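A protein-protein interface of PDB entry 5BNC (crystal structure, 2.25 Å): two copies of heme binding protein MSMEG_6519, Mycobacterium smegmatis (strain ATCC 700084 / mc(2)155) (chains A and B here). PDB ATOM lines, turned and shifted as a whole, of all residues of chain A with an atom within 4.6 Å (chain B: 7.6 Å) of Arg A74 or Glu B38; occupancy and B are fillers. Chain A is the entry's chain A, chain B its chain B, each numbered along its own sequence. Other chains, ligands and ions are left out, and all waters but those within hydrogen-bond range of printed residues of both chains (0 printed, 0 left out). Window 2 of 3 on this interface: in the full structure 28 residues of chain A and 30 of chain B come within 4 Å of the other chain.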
ATOM      1  N   ALA A  33      32.727  11.060  -5.564  1.00  0.00           N
ATOM      2  CA  ALA A  33      31.282  11.264  -5.470  1.00  0.00           C
ATOM      3  C   ALA A  33      31.035  12.696  -5.852  1.00  0.00           C
ATOM      4  O   ALA A  33      31.649  13.623  -5.285  1.00  0.00           O
ATOM      5  CB  ALA A  33      30.742  10.959  -4.060  1.00  0.00           C
ATOM      6  N   THR A  34      30.165  12.868  -6.830  1.00  0.00           N
ATOM      7  CA  THR A  34      29.738  14.192  -7.276  1.00  0.00           C
ATOM      8  C   THR A  34      28.221  14.219  -7.391  1.00  0.00           C
ATOM      9  O   THR A  34      27.545  13.217  -7.138  1.00  0.00           O
ATOM     10  CB  THR A  34      30.372  14.570  -8.605  1.00  0.00           C
ATOM     11  OG1 THR A  34      29.988  13.624  -9.605  1.00  0.00           O
ATOM     12  CG2 THR A  34      31.873  14.603  -8.496  1.00  0.00           C
ATOM     13  N   LEU A  35      27.694  15.399  -7.684  1.00  0.00           N
ATOM     14  CA  LEU A  35      26.261  15.632  -7.856  1.00  0.00           C
ATOM     15  C   LEU A  35      25.955  15.744  -9.337  1.00  0.00           C
ATOM     16  O   LEU A  35      26.603  16.516 -10.007  1.00  0.00           O
ATOM     17  CB  LEU A  35      25.871  16.972  -7.209  1.00  0.00           C
ATOM     18  CG  LEU A  35      26.117  17.033  -5.713  1.00  0.00           C
ATOM     19  CD1 LEU A  35      25.769  18.400  -5.146  1.00  0.00           C
ATOM     20  CD2 LEU A  35      25.318  15.963  -4.993  1.00  0.00           C
ATOM     21  N   LEU A  69      31.284  18.548 -11.687  1.00  0.00           N
ATOM     22  CA  LEU A  69      32.129  19.464 -10.936  1.00  0.00           C
ATOM     23  C   LEU A  69      31.981  20.910 -11.425  1.00  0.00           C
ATOM     24  O   LEU A  69      31.977  21.853 -10.609  1.00  0.00           O
ATOM     25  CB  LEU A  69      33.610  19.039 -11.010  1.00  0.00           C
ATOM     26  CG  LEU A  69      34.030  17.780 -10.241  1.00  0.00           C
ATOM     27  CD1 LEU A  69      35.483  17.488 -10.489  1.00  0.00           C
ATOM     28  CD2 LEU A  69      33.783  17.955  -8.759  1.00  0.00           C
ATOM     29  N   ASP A  72      28.656  22.055  -9.904  1.00  0.00           N
ATOM     30  CA  ASP A  72      28.665  22.162  -8.461  1.00  0.00           C
ATOM     31  C   ASP A  72      29.936  21.486  -7.971  1.00  0.00           C
ATOM     32  O   ASP A  72      30.102  20.264  -8.112  1.00  0.00           O
ATOM     33  CB  ASP A  72      27.449  21.517  -7.890  1.00  0.00           C
ATOM     34  CG  ASP A  72      27.367  21.682  -6.406  1.00  0.00           C
ATOM     35  OD1 ASP A  72      28.412  21.910  -5.796  1.00  0.00           O
ATOM     36  OD2 ASP A  72      26.250  21.623  -5.858  1.00  0.00           O
ATOM     37  N   PRO A  73      30.873  22.286  -7.452  1.00  0.00           N
ATOM     38  CA  PRO A  73      32.187  21.733  -7.228  1.00  0.00           C
ATOM     39  C   PRO A  73      32.328  20.916  -5.937  1.00  0.00           C
ATOM     40  O   PRO A  73      33.400  20.416  -5.641  1.00  0.00           O
ATOM     41  CB  PRO A  73      33.082  22.989  -7.240  1.00  0.00           C
ATOM     42  CG  PRO A  73      32.215  24.033  -6.645  1.00  0.00           C
ATOM     43  CD  PRO A  73      30.797  23.708  -7.054  1.00  0.00           C
ATOM     44  N   ARG A  74      31.262  20.722  -5.183  1.00  0.00           N
ATOM     45  CA  ARG A  74      31.296  19.763  -4.058  1.00  0.00           C
ATOM     46  C   ARG A  74      31.619  18.363  -4.539  1.00  0.00           C
ATOM     47  O   ARG A  74      30.985  17.858  -5.458  1.00  0.00           O
ATOM     48  CB  ARG A  74      29.987  19.725  -3.325  1.00  0.00           C
ATOM     49  CG  ARG A  74      29.783  20.996  -2.522  1.00  0.00           C
ATOM     50  CD  ARG A  74      28.373  21.499  -2.737  1.00  0.00           C
ATOM     51  NE  ARG A  74      27.399  21.061  -1.779  1.00  0.00           N
ATOM     52  CZ  ARG A  74      26.095  20.924  -2.015  1.00  0.00           C
ATOM     53  NH1 ARG A  74      25.587  21.138  -3.202  1.00  0.00           N
ATOM     54  NH2 ARG A  74      25.312  20.560  -1.030  1.00  0.00           N
ATOM     55  N   ALA A  75      32.593  17.757  -3.898  1.00  0.00           N
ATOM     56  CA  ALA A  75      33.020  16.418  -4.214  1.00  0.00           C
ATOM     57  C   ALA A  75      33.595  15.739  -2.968  1.00  0.00           C
ATOM     58  O   ALA A  75      34.050  16.413  -2.037  1.00  0.00           O
ATOM     59  CB  ALA A  75      34.064  16.472  -5.289  1.00  0.00           C
ATOM     60  N   GLY A  98      35.168  17.720   0.297  1.00  0.00           N
ATOM     61  CA  GLY A  98      35.161  19.168   0.238  1.00  0.00           C
ATOM     62  C   GLY A  98      34.668  19.715  -1.073  1.00  0.00           C
ATOM     63  O   GLY A  98      33.539  19.435  -1.479  1.00  0.00           O
ATOM     64  N   VAL A  99      35.548  20.472  -1.715  1.00  0.00           N
ATOM     65  CA  VAL A  99      35.202  21.338  -2.832  1.00  0.00           C
ATOM     66  C   VAL A  99      36.368  21.316  -3.815  1.00  0.00           C
ATOM     67  O   VAL A  99      37.480  21.620  -3.415  1.00  0.00           O
ATOM     68  CB  VAL A  99      34.914  22.784  -2.276  1.00  0.00           C
ATOM     69  CG1 VAL A  99      35.341  23.891  -3.207  1.00  0.00           C
ATOM     70  CG2 VAL A  99      33.448  22.944  -1.936  1.00  0.00           C
ATOM     71  N   LEU B  35      23.947  11.131  -0.544  1.00  0.00           N
ATOM     72  CA  LEU B  35      23.760  12.543  -0.267  1.00  0.00           C
ATOM     73  C   LEU B  35      23.712  12.745   1.221  1.00  0.00           C
ATOM     74  O   LEU B  35      23.029  12.008   1.924  1.00  0.00           O
ATOM     75  CB  LEU B  35      22.426  12.973  -0.836  1.00  0.00           C
ATOM     76  CG  LEU B  35      22.252  12.904  -2.351  1.00  0.00           C
ATOM     77  CD1 LEU B  35      20.866  13.378  -2.799  1.00  0.00           C
ATOM     78  CD2 LEU B  35      23.310  13.755  -3.022  1.00  0.00           C
ATOM     79  N   THR B  36      24.461  13.692   1.734  1.00  0.00           N
ATOM     80  CA  THR B  36      24.279  14.082   3.154  1.00  0.00           C
ATOM     81  C   THR B  36      22.968  14.856   3.203  1.00  0.00           C
ATOM     82  O   THR B  36      22.360  15.138   2.143  1.00  0.00           O
ATOM     83  CB  THR B  36      25.400  15.007   3.701  1.00  0.00           C
ATOM     84  OG1 THR B  36      25.299  16.302   3.088  1.00  0.00           O
ATOM     85  CG2 THR B  36      26.777  14.453   3.408  1.00  0.00           C
ATOM     86  N   THR B  37      22.534  15.257   4.404  1.00  0.00           N
ATOM     87  CA  THR B  37      21.257  15.952   4.521  1.00  0.00           C
ATOM     88  C   THR B  37      21.347  17.294   3.880  1.00  0.00           C
ATOM     89  O   THR B  37      20.305  17.850   3.456  1.00  0.00           O
ATOM     90  CB  THR B  37      20.891  16.330   5.935  1.00  0.00           C
ATOM     91  OG1 THR B  37      21.939  17.197   6.388  1.00  0.00           O
ATOM     92  CG2 THR B  37      20.737  15.080   6.825  1.00  0.00           C
ATOM     93  N   GLU B  38      22.556  17.865   3.808  1.00  0.00           N
ATOM     94  CA  GLU B  38      22.748  19.157   3.130  1.00  0.00           C
ATOM     95  C   GLU B  38      22.937  19.014   1.626  1.00  0.00           C
ATOM     96  O   GLU B  38      23.229  19.999   0.926  1.00  0.00           O
ATOM     97  CB  GLU B  38      23.945  19.912   3.708  1.00  0.00           C
ATOM     98  CG  GLU B  38      24.009  19.988   5.231  1.00  0.00           C
ATOM     99  CD  GLU B  38      25.038  20.999   5.685  1.00  0.00           C
ATOM    100  OE1 GLU B  38      26.215  20.864   5.295  1.00  0.00           O
ATOM    101  OE2 GLU B  38      24.656  21.935   6.401  1.00  0.00           O
ATOM    102  N   GLY B  39      22.788  17.793   1.113  1.00  0.00           N
ATOM    103  CA  GLY B  39      22.963  17.555  -0.317  1.00  0.00           C
ATOM    104  C   GLY B  39      24.426  17.527  -0.798  1.00  0.00           C
ATOM    105  O   GLY B  39      24.673  17.714  -1.987  1.00  0.00           O
ATOM    106  N   ASP B  40      25.395  17.292   0.087  1.00  0.00           N
ATOM    107  CA  ASP B  40      26.793  17.114  -0.347  1.00  0.00           C
ATOM    108  C   ASP B  40      26.998  15.692  -0.806  1.00  0.00           C
ATOM    109  O   ASP B  40      26.423  14.777  -0.228  1.00  0.00           O
ATOM    110  CB  ASP B  40      27.798  17.320   0.762  1.00  0.00           C
ATOM    111  CG  ASP B  40      27.762  18.708   1.377  1.00  0.00           C
ATOM    112  OD1 ASP B  40      27.305  19.676   0.725  1.00  0.00           O
ATOM    113  OD2 ASP B  40      28.300  18.800   2.509  1.00  0.00           O
ATOM    114  N   PRO B  41      27.840  15.493  -1.827  1.00  0.00           N
ATOM    115  CA  PRO B  41      28.077  14.123  -2.296  1.00  0.00           C
ATOM    116  C   PRO B  41      29.071  13.395  -1.372  1.00  0.00           C
ATOM    117  O   PRO B  41      30.159  13.910  -1.127  1.00  0.00           O
ATOM    118  CB  PRO B  41      28.610  14.346  -3.727  1.00  0.00           C
ATOM    119  CG  PRO B  41      29.330  15.644  -3.659  1.00  0.00           C
ATOM    120  CD  PRO B  41      28.556  16.486  -2.656  1.00  0.00           C
ATOM    121  N   ASN B  68      22.473   8.584   5.504  1.00  0.00           N
ATOM    122  CA  ASN B  68      22.157   9.270   4.267  1.00  0.00           C
ATOM    123  C   ASN B  68      21.008   8.540   3.560  1.00  0.00           C
ATOM    124  O   ASN B  68      20.040   9.169   3.129  1.00  0.00           O
ATOM    125  CB  ASN B  68      23.377   9.419   3.377  1.00  0.00           C
ATOM    126  CG  ASN B  68      24.409  10.368   3.951  1.00  0.00           C
ATOM    127  OD1 ASN B  68      24.117  11.117   4.821  1.00  0.00           O
ATOM    128  ND2 ASN B  68      25.645  10.271   3.494  1.00  0.00           N
ATOM    129  N   HIS B  71      17.585   9.106   4.991  1.00  0.00           N
ATOM    130  CA  HIS B  71      17.086  10.437   4.744  1.00  0.00           C
ATOM    131  C   HIS B  71      16.732  10.672   3.267  1.00  0.00           C
ATOM    132  O   HIS B  71      15.726  11.298   2.960  1.00  0.00           O
ATOM    133  CB  HIS B  71      18.096  11.478   5.211  1.00  0.00           C
ATOM    134  CG  HIS B  71      17.767  12.885   4.766  1.00  0.00           C
ATOM    135  ND1 HIS B  71      16.931  13.720   5.480  1.00  0.00           N
ATOM    136  CD2 HIS B  71      18.173  13.605   3.690  1.00  0.00           C
ATOM    137  CE1 HIS B  71      16.813  14.875   4.852  1.00  0.00           C
ATOM    138  NE2 HIS B  71      17.570  14.836   3.770  1.00  0.00           N
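The guanidinium group (NH2) of Arg A74 is in hydrogen-bond range of the backbone carbonyl oxygen (O) of Glu B38, 2.9 Å away.
NH2 of Arg A74 is in hydrogen-bond range of O of Gly B39 (3.1 Å).
OD1 of Asp B40 lies within salt-bridge range of NH2 of Arg A74 (2.8 Å).
The guanidinium group of Arg A74 is in salt-bridge range of the side-chain carboxylate of Asp A72 (2.8 Å).
The backbone carbonyl oxygen (O) of Ala A75 sits at hydrogen-bond distance from the backbone NH (N) of Gly A98 (2.9 Å).
The side-chain amide oxygen (OD1) of Asn B68 lies close to the backbone carbonyl oxygen (O) of Leu B35, 3.2 Å away.
OG1 of Thr B36 sits close to N of Glu B38, 3.2 Å away.
The backbone NH of Asp B40 lies within hydrogen-bond range of the side-chain hydroxyl of Thr B36 (3.2 Å).
Among the printed residues, merely in contact across the chains: Ala A33 with Pro B41 (3.5 Å), Thr A34 with Pro B41 (3.7 Å), Leu A35 with Leu B35 (3.6 Å), Leu A35 with Gly B39 (3.4 Å), Leu A35 with Pro B41 (3.9 Å), Arg A74 with Pro B41 (3.3 Å) and Ala A75 with Pro B41 (3.8 Å).
Of the printed residues of chain B, Arg A74 touches Glu B38, Gly B39, Asp B40 and Pro B41.
Of the printed residues of chain B, Thr A34 touches Pro B41 (3.7 Å).
Of the printed residues of chain A, Asp B40 touches Arg A74 (2.8 Å).
Of the printed residues of chain A, Pro B41 touches Ala A33 (3.5 Å), Thr A34 (3.7 Å), Leu A35 (3.9 Å), Arg A74 (3.3 Å) and Ala A75 (3.8 Å).
Printed residues of chain B within 4 Å of Ala A75: Pro B41.
Printed residues of chain B within 4 Å of Leu A35: Leu B35 (3.6 Å), Gly B39 (3.4 Å) and Pro B41 (3.9 Å).
His B71 touches none of the printed residues of chain A.
Gly A98 touches none of the printed residues of chain B.
The nearest printed residue of chain B that does not touch Arg A74 is Thr B36 (5.9 Å).
The nearest printed residue of chain A that does not touch Glu B38 is Leu A35 (6.8 Å).
Printed residues of chain A that touch a printed residue of chain B: Ala A33, Thr A34, Leu A35, Arg A74 and Ala A75.
Hydrophobic or aromatic side chains of chain A within 4 Å of the printed part of chain B: Ala A33 and Leu A35.
Printed residues of chain B that touch a printed residue of chain A: Leu B35, Glu B38, Gly B39, Asp B40 and Pro B41.
Among the printed residues, 10 pairs touch across the chains.
Among the printed residues, Asp or Glu carboxylates within 4 Å of a Lys or Arg side-chain nitrogen of the other chain: Arg A74 with Asp B40 (2.8 Å).
Leu A35 touches its own counterpart, Leu B35.
Position printed for both chains: 35.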
